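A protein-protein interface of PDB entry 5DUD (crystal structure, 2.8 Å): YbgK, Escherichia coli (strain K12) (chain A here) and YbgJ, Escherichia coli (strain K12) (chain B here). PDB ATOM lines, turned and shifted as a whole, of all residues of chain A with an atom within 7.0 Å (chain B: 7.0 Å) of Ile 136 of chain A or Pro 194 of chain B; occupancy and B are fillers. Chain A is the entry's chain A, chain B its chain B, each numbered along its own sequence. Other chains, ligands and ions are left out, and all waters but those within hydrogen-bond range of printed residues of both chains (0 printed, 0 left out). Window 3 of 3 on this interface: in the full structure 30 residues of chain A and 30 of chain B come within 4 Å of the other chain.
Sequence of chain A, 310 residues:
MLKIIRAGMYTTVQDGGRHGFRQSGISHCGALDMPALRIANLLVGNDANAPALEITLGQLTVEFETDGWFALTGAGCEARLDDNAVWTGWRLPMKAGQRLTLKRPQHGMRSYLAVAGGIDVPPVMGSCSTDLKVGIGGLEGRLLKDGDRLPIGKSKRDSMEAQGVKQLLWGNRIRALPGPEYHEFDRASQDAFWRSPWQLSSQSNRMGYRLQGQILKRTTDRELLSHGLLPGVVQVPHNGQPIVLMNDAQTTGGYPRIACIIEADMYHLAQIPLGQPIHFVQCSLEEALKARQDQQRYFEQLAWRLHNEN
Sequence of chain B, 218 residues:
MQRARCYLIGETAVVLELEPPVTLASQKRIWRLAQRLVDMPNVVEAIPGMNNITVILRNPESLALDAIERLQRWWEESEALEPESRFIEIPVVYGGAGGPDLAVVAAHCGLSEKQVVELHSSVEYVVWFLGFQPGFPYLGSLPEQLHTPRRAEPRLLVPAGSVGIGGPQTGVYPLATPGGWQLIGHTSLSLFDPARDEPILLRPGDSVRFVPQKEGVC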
ATOM      1  N   ARG A  18      14.890 -21.830   9.637  1.00  0.00           N
ATOM      2  CA  ARG A  18      15.343 -22.583   8.470  1.00  0.00           C
ATOM      3  C   ARG A  18      16.883 -22.494   8.402  1.00  0.00           C
ATOM      4  O   ARG A  18      17.428 -21.713   7.630  1.00  0.00           O
ATOM      5  CB  ARG A  18      14.651 -22.011   7.218  1.00  0.00           C
ATOM      6  CG  ARG A  18      14.841 -22.843   5.962  1.00  0.00           C
ATOM      7  CD  ARG A  18      13.927 -22.446   4.816  1.00  0.00           C
ATOM      8  NE  ARG A  18      12.530 -22.819   5.064  1.00  0.00           N
ATOM      9  CZ  ARG A  18      11.568 -22.026   5.542  1.00  0.00           C
ATOM     10  NH1 ARG A  18      11.828 -20.754   5.845  1.00  0.00           N
ATOM     11  NH2 ARG A  18      10.341 -22.495   5.726  1.00  0.00           N
ATOM     12  N   ILE A  26      19.587 -17.965   1.804  1.00  0.00           N
ATOM     13  CA  ILE A  26      18.287 -18.164   2.455  1.00  0.00           C
ATOM     14  C   ILE A  26      18.369 -17.676   3.900  1.00  0.00           C
ATOM     15  O   ILE A  26      19.205 -18.156   4.666  1.00  0.00           O
ATOM     16  CB  ILE A  26      17.835 -19.658   2.365  1.00  0.00           C
ATOM     17  CG1 ILE A  26      17.410 -19.994   0.926  1.00  0.00           C
ATOM     18  CG2 ILE A  26      16.694 -19.978   3.370  1.00  0.00           C
ATOM     19  CD1 ILE A  26      17.562 -21.497   0.474  1.00  0.00           C
ATOM     20  N   SER A  27      17.467 -16.756   4.282  1.00  0.00           N
ATOM     21  CA  SER A  27      17.381 -16.227   5.644  1.00  0.00           C
ATOM     22  C   SER A  27      16.768 -17.293   6.551  1.00  0.00           C
ATOM     23  O   SER A  27      15.892 -18.027   6.096  1.00  0.00           O
ATOM     24  CB  SER A  27      16.543 -14.953   5.659  1.00  0.00           C
ATOM     25  OG  SER A  27      16.889 -14.089   4.588  1.00  0.00           O
ATOM     26  N   VAL A 124       9.073 -26.907   4.831  1.00  0.00           N
ATOM     27  CA  VAL A 124       9.855 -26.594   3.640  1.00  0.00           C
ATOM     28  C   VAL A 124      11.321 -26.397   4.037  1.00  0.00           C
ATOM     29  O   VAL A 124      11.667 -25.348   4.586  1.00  0.00           O
ATOM     30  CB  VAL A 124       9.286 -25.347   2.912  1.00  0.00           C
ATOM     31  CG1 VAL A 124      10.184 -24.941   1.741  1.00  0.00           C
ATOM     32  CG2 VAL A 124       7.856 -25.596   2.439  1.00  0.00           C
ATOM     33  N   MET A 125      12.169 -27.413   3.751  1.00  0.00           N
ATOM     34  CA  MET A 125      13.604 -27.424   4.043  1.00  0.00           C
ATOM     35  C   MET A 125      13.853 -27.393   5.572  1.00  0.00           C
ATOM     36  O   MET A 125      14.482 -26.481   6.104  1.00  0.00           O
ATOM     37  CB  MET A 125      14.330 -26.292   3.282  1.00  0.00           C
ATOM     38  CG  MET A 125      14.663 -26.670   1.851  1.00  0.00           C
ATOM     39  SD  MET A 125      15.238 -25.297   0.825  1.00  0.00           S
ATOM     40  CE  MET A 125      13.808 -24.261   0.833  1.00  0.00           C
ATOM     41  N   CYS A 128       9.107 -24.695   9.115  1.00  0.00           N
ATOM     42  CA  CYS A 128       7.778 -24.210   8.746  1.00  0.00           C
ATOM     43  C   CYS A 128       7.703 -22.671   8.855  1.00  0.00           C
ATOM     44  O   CYS A 128       6.610 -22.108   8.768  1.00  0.00           O
ATOM     45  CB  CYS A 128       6.729 -24.878   9.628  1.00  0.00           C
ATOM     46  SG  CYS A 128       6.834 -26.687   9.664  1.00  0.00           S
ATOM     47  N   SER A 129       8.858 -21.989   9.005  1.00  0.00           N
ATOM     48  CA  SER A 129       8.897 -20.530   9.105  1.00  0.00           C
ATOM     49  C   SER A 129       8.516 -19.882   7.788  1.00  0.00           C
ATOM     50  O   SER A 129       9.068 -20.237   6.746  1.00  0.00           O
ATOM     51  CB  SER A 129      10.284 -20.055   9.517  1.00  0.00           C
ATOM     52  OG  SER A 129      10.568 -20.447  10.848  1.00  0.00           O
ATOM     53  N   THR A 130       7.615 -18.895   7.841  1.00  0.00           N
ATOM     54  CA  THR A 130       7.130 -18.203   6.649  1.00  0.00           C
ATOM     55  C   THR A 130       8.144 -17.166   6.182  1.00  0.00           C
ATOM     56  O   THR A 130       8.505 -16.272   6.952  1.00  0.00           O
ATOM     57  CB  THR A 130       5.775 -17.528   6.920  1.00  0.00           C
ATOM     58  OG1 THR A 130       4.956 -18.403   7.692  1.00  0.00           O
ATOM     59  CG2 THR A 130       5.038 -17.156   5.642  1.00  0.00           C
ATOM     60  N   ASP A 131       8.603 -17.293   4.929  1.00  0.00           N
ATOM     61  CA  ASP A 131       9.518 -16.343   4.301  1.00  0.00           C
ATOM     62  C   ASP A 131       8.678 -15.508   3.330  1.00  0.00           C
ATOM     63  O   ASP A 131       8.277 -16.003   2.276  1.00  0.00           O
ATOM     64  CB  ASP A 131      10.669 -17.096   3.613  1.00  0.00           C
ATOM     65  CG  ASP A 131      11.920 -16.265   3.377  1.00  0.00           C
ATOM     66  OD1 ASP A 131      11.809 -15.020   3.330  1.00  0.00           O
ATOM     67  OD2 ASP A 131      13.006 -16.861   3.209  1.00  0.00           O
ATOM     68  N   LEU A 132       8.339 -14.276   3.729  1.00  0.00           N
ATOM     69  CA  LEU A 132       7.450 -13.402   2.959  1.00  0.00           C
ATOM     70  C   LEU A 132       8.124 -12.800   1.720  1.00  0.00           C
ATOM     71  O   LEU A 132       7.422 -12.485   0.761  1.00  0.00           O
ATOM     72  CB  LEU A 132       6.910 -12.278   3.854  1.00  0.00           C
ATOM     73  CG  LEU A 132       6.091 -12.741   5.063  1.00  0.00           C
ATOM     74  CD1 LEU A 132       6.077 -11.683   6.146  1.00  0.00           C
ATOM     75  CD2 LEU A 132       4.674 -13.106   4.667  1.00  0.00           C
ATOM     76  N   LYS A 133       9.462 -12.648   1.732  1.00  0.00           N
ATOM     77  CA  LYS A 133      10.209 -12.118   0.585  1.00  0.00           C
ATOM     78  C   LYS A 133      10.406 -13.198  -0.481  1.00  0.00           C
ATOM     79  O   LYS A 133      10.335 -12.899  -1.671  1.00  0.00           O
ATOM     80  CB  LYS A 133      11.574 -11.580   1.041  1.00  0.00           C
ATOM     81  CG  LYS A 133      12.450 -11.015  -0.082  1.00  0.00           C
ATOM     82  CD  LYS A 133      13.561 -10.138   0.474  1.00  0.00           C
ATOM     83  CE  LYS A 133      14.583  -9.737  -0.567  1.00  0.00           C
ATOM     84  NZ  LYS A 133      14.015  -8.861  -1.631  1.00  0.00           N
ATOM     85  N   VAL A 134      10.649 -14.444  -0.045  1.00  0.00           N
ATOM     86  CA  VAL A 134      10.890 -15.591  -0.924  1.00  0.00           C
ATOM     87  C   VAL A 134       9.573 -16.263  -1.338  1.00  0.00           C
ATOM     88  O   VAL A 134       9.496 -16.814  -2.435  1.00  0.00           O
ATOM     89  CB  VAL A 134      11.843 -16.600  -0.237  1.00  0.00           C
ATOM     90  CG1 VAL A 134      12.132 -17.802  -1.124  1.00  0.00           C
ATOM     91  CG2 VAL A 134      13.145 -15.923   0.192  1.00  0.00           C
ATOM     92  N   GLY A 135       8.577 -16.261  -0.454  1.00  0.00           N
ATOM     93  CA  GLY A 135       7.282 -16.883  -0.712  1.00  0.00           C
ATOM     94  C   GLY A 135       7.269 -18.378  -0.478  1.00  0.00           C
ATOM     95  O   GLY A 135       6.777 -19.129  -1.322  1.00  0.00           O
ATOM     96  N   ILE A 136       7.811 -18.824   0.678  1.00  0.00           N
ATOM     97  CA  ILE A 136       7.865 -20.242   1.064  1.00  0.00           C
ATOM     98  C   ILE A 136       7.548 -20.407   2.554  1.00  0.00           C
ATOM     99  O   ILE A 136       7.640 -19.449   3.322  1.00  0.00           O
ATOM    100  CB  ILE A 136       9.243 -20.878   0.729  1.00  0.00           C
ATOM    101  CG1 ILE A 136      10.408 -20.119   1.409  1.00  0.00           C
ATOM    102  CG2 ILE A 136       9.445 -20.951  -0.778  1.00  0.00           C
ATOM    103  CD1 ILE A 136      11.723 -20.896   1.464  1.00  0.00           C
ATOM    104  N   GLY A 137       7.197 -21.629   2.947  1.00  0.00           N
ATOM    105  CA  GLY A 137       6.900 -21.966   4.332  1.00  0.00           C
ATOM    106  C   GLY A 137       5.563 -21.472   4.838  1.00  0.00           C
ATOM    107  O   GLY A 137       4.925 -20.623   4.213  1.00  0.00           O
ATOM    108  N   GLY A 138       5.164 -22.002   5.991  1.00  0.00           N
ATOM    109  CA  GLY A 138       3.908 -21.670   6.653  1.00  0.00           C
ATOM    110  C   GLY A 138       2.694 -22.105   5.860  1.00  0.00           C
ATOM    111  O   GLY A 138       2.508 -23.301   5.623  1.00  0.00           O
ATOM    112  N   LEU A 139       1.884 -21.136   5.425  1.00  0.00           N
ATOM    113  CA  LEU A 139       0.704 -21.396   4.614  1.00  0.00           C
ATOM    114  C   LEU A 139       0.860 -20.658   3.290  1.00  0.00           C
ATOM    115  O   LEU A 139       0.481 -19.490   3.173  1.00  0.00           O
ATOM    116  CB  LEU A 139      -0.572 -20.977   5.361  1.00  0.00           C
ATOM    117  N   GLU A 140       1.490 -21.337   2.308  1.00  0.00           N
ATOM    118  CA  GLU A 140       1.732 -20.855   0.941  1.00  0.00           C
ATOM    119  C   GLU A 140       2.708 -19.644   0.858  1.00  0.00           C
ATOM    120  O   GLU A 140       2.809 -19.022  -0.201  1.00  0.00           O
ATOM    121  CB  GLU A 140       0.401 -20.495   0.246  1.00  0.00           C
ATOM    122  CG  GLU A 140      -0.649 -21.599   0.308  1.00  0.00           C
ATOM    123  CD  GLU A 140      -1.987 -21.273  -0.328  1.00  0.00           C
ATOM    124  OE1 GLU A 140      -2.190 -20.113  -0.753  1.00  0.00           O
ATOM    125  OE2 GLU A 140      -2.845 -22.183  -0.385  1.00  0.00           O
ATOM    126  N   GLY A 141       3.461 -19.370   1.927  1.00  0.00           N
ATOM    127  CA  GLY A 141       4.416 -18.266   1.954  1.00  0.00           C
ATOM    128  C   GLY A 141       3.782 -16.891   1.905  1.00  0.00           C
ATOM    129  O   GLY A 141       4.176 -16.061   1.083  1.00  0.00           O
ATOM    130  N   ARG A 142       2.791 -16.649   2.770  1.00  0.00           N
ATOM    131  CA  ARG A 142       2.079 -15.371   2.820  1.00  0.00           C
ATOM    132  C   ARG A 142       1.473 -15.123   4.203  1.00  0.00           C
ATOM    133  O   ARG A 142       1.461 -16.020   5.045  1.00  0.00           O
ATOM    134  CB  ARG A 142       0.971 -15.339   1.745  1.00  0.00           C
ATOM    135  CG  ARG A 142       0.028 -16.547   1.762  1.00  0.00           C
ATOM    136  CD  ARG A 142      -1.285 -16.244   1.054  1.00  0.00           C
ATOM    137  NE  ARG A 142      -2.214 -17.374   1.112  1.00  0.00           N
ATOM    138  CZ  ARG A 142      -2.997 -17.675   2.147  1.00  0.00           C
ATOM    139  NH1 ARG A 142      -2.966 -16.938   3.256  1.00  0.00           N
ATOM    140  NH2 ARG A 142      -3.801 -18.729   2.091  1.00  0.00           N
ATOM    141  N   PRO B 134      17.746 -16.134  -2.268  1.00  0.00           N
ATOM    142  CA  PRO B 134      18.025 -17.569  -2.394  1.00  0.00           C
ATOM    143  C   PRO B 134      18.528 -17.996  -3.782  1.00  0.00           C
ATOM    144  O   PRO B 134      17.792 -17.909  -4.763  1.00  0.00           O
ATOM    145  CB  PRO B 134      16.655 -18.202  -2.101  1.00  0.00           C
ATOM    146  CG  PRO B 134      15.970 -17.228  -1.247  1.00  0.00           C
ATOM    147  CD  PRO B 134      16.343 -15.924  -1.866  1.00  0.00           C
ATOM    148  N   PHE B 192      16.496 -21.225  -7.994  1.00  0.00           N
ATOM    149  CA  PHE B 192      15.990 -21.572  -6.670  1.00  0.00           C
ATOM    150  C   PHE B 192      14.587 -22.134  -6.830  1.00  0.00           C
ATOM    151  O   PHE B 192      13.706 -21.426  -7.315  1.00  0.00           O
ATOM    152  CB  PHE B 192      15.990 -20.349  -5.752  1.00  0.00           C
ATOM    153  CG  PHE B 192      15.182 -20.532  -4.490  1.00  0.00           C
ATOM    154  CD1 PHE B 192      15.620 -21.376  -3.486  1.00  0.00           C
ATOM    155  CD2 PHE B 192      13.969 -19.888  -4.325  1.00  0.00           C
ATOM    156  CE1 PHE B 192      14.865 -21.563  -2.329  1.00  0.00           C
ATOM    157  CE2 PHE B 192      13.212 -20.080  -3.168  1.00  0.00           C
ATOM    158  CZ  PHE B 192      13.666 -20.911  -2.174  1.00  0.00           C
ATOM    159  N   ASP B 193      14.402 -23.405  -6.458  1.00  0.00           N
ATOM    160  CA  ASP B 193      13.121 -24.103  -6.505  1.00  0.00           C
ATOM    161  C   ASP B 193      12.950 -24.757  -5.139  1.00  0.00           C
ATOM    162  O   ASP B 193      13.773 -25.589  -4.770  1.00  0.00           O
ATOM    163  CB  ASP B 193      13.101 -25.127  -7.657  1.00  0.00           C
ATOM    164  CG  ASP B 193      11.728 -25.643  -8.066  1.00  0.00           C
ATOM    165  OD1 ASP B 193      10.772 -25.485  -7.281  1.00  0.00           O
ATOM    166  OD2 ASP B 193      11.609 -26.203  -9.179  1.00  0.00           O
ATOM    167  N   PRO B 194      11.953 -24.365  -4.327  1.00  0.00           N
ATOM    168  CA  PRO B 194      11.850 -24.947  -2.978  1.00  0.00           C
ATOM    169  C   PRO B 194      11.376 -26.419  -2.896  1.00  0.00           C
ATOM    170  O   PRO B 194      11.672 -27.027  -1.866  1.00  0.00           O
ATOM    171  CB  PRO B 194      10.872 -24.004  -2.272  1.00  0.00           C
ATOM    172  CG  PRO B 194      10.042 -23.428  -3.355  1.00  0.00           C
ATOM    173  CD  PRO B 194      10.910 -23.347  -4.564  1.00  0.00           C
ATOM    174  N   ALA B 195      10.807 -27.042  -3.981  1.00  0.00           N
ATOM    175  CA  ALA B 195      10.339 -28.447  -3.957  1.00  0.00           C
ATOM    176  C   ALA B 195      11.084 -29.415  -4.916  1.00  0.00           C
ATOM    177  O   ALA B 195      10.623 -30.547  -5.061  1.00  0.00           O
ATOM    178  CB  ALA B 195       8.847 -28.486  -4.296  1.00  0.00           C
ATOM    179  N   ARG B 196      12.212 -29.031  -5.540  1.00  0.00           N
ATOM    180  CA  ARG B 196      12.871 -29.936  -6.511  1.00  0.00           C
ATOM    181  C   ARG B 196      13.436 -31.272  -5.903  1.00  0.00           C
ATOM    182  O   ARG B 196      12.819 -32.318  -6.101  1.00  0.00           O
ATOM    183  CB  ARG B 196      13.977 -29.210  -7.299  1.00  0.00           C
ATOM    184  N   ASP B 197      14.584 -31.227  -5.199  1.00  0.00           N
ATOM    185  CA  ASP B 197      15.356 -32.349  -4.592  1.00  0.00           C
ATOM    186  C   ASP B 197      16.655 -31.724  -4.061  1.00  0.00           C
ATOM    187  O   ASP B 197      16.996 -31.876  -2.892  1.00  0.00           O
ATOM    188  CB  ASP B 197      15.640 -33.506  -5.579  1.00  0.00           C
ATOM    189  N   PRO B 199      17.426 -27.966  -3.805  1.00  0.00           N
ATOM    190  CA  PRO B 199      16.684 -26.721  -4.052  1.00  0.00           C
ATOM    191  C   PRO B 199      17.465 -25.615  -4.758  1.00  0.00           C
ATOM    192  O   PRO B 199      16.886 -24.955  -5.618  1.00  0.00           O
ATOM    193  CB  PRO B 199      16.226 -26.285  -2.660  1.00  0.00           C
ATOM    194  CG  PRO B 199      17.060 -27.036  -1.701  1.00  0.00           C
ATOM    195  CD  PRO B 199      17.491 -28.289  -2.365  1.00  0.00           C
ATOM    196  N   ILE B 200      18.740 -25.415  -4.409  1.00  0.00           N
ATOM    197  CA  ILE B 200      19.571 -24.380  -5.036  1.00  0.00           C
ATOM    198  C   ILE B 200      20.411 -25.063  -6.100  1.00  0.00           C
ATOM    199  O   ILE B 200      21.069 -26.068  -5.820  1.00  0.00           O
ATOM    200  CB  ILE B 200      20.412 -23.616  -3.981  1.00  0.00           C
ATOM    201  CG1 ILE B 200      19.484 -23.027  -2.893  1.00  0.00           C
ATOM    202  CG2 ILE B 200      21.223 -22.494  -4.658  1.00  0.00           C
ATOM    203  CD1 ILE B 200      19.432 -23.808  -1.597  1.00  0.00           C
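N of Asp 131 of chain A lies within hydrogen-bond range of O of Ile 136 of chain A. N of Asp 193 of chain B lies within hydrogen-bond range of O of Pro 199 of chain B, 3.0 Å away.
Among the printed residues, pairs that only touch across the chains: Val 134 of chain A with Phe 192 of chain B (3.2 Å), Val 134 of chain A with Pro 134 of chain B (3.4 Å), Met 125 of chain A with Pro 199 of chain B (3.6 Å), Ile 26 of chain A with Pro 134 of chain B (3.6 Å), Ile 26 of chain A with Ile 200 of chain B (3.6 Å), Ile 136 of chain A with Pro 194 of chain B (3.6 Å) and Ile 26 of chain A with Phe 192 of chain B (3.9 Å).
Of the printed residues of chain B, Met 125 of chain A touches Pro 199 (3.6 Å). Leu 132 of chain A touches none of the printed residues of chain B. Printed residues of chain B within 4 Å of Val 134 of chain A: Pro 134 and Phe 192. No residue of chain B comes within 4 Å of Gly 135 of chain A. Of the printed residues of chain A, Pro 134 of chain B touches Ile 26 and Val 134. Pro 194 of chain B touches just one residue of chain A: Ile 136 (3.6 Å). Of the printed residues of chain A, Pro 199 of chain B touches Met 125 (3.6 Å). Printed residues of chain A within 4 Å of Ile 200 of chain B: Ile 26. The nearest residue of chain A that does not touch Pro 194 of chain B is Val 124 of chain A (4.2 Å).
Hydrophobic or aromatic side chains of chain A within 4 Å of the printed part of chain B: Ile 26, Met 125, Val 134 and Ile 136. Of the 9 printed residues of chain B, 5 touch a printed residue of chain A. Hydrophobic or aromatic side chains of chain B within 4 Å of the printed part of chain A: Pro 134, Phe 192, Pro 194, Pro 199 and Ile 200. Among the printed residues, 7 pairs touch across the chains.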
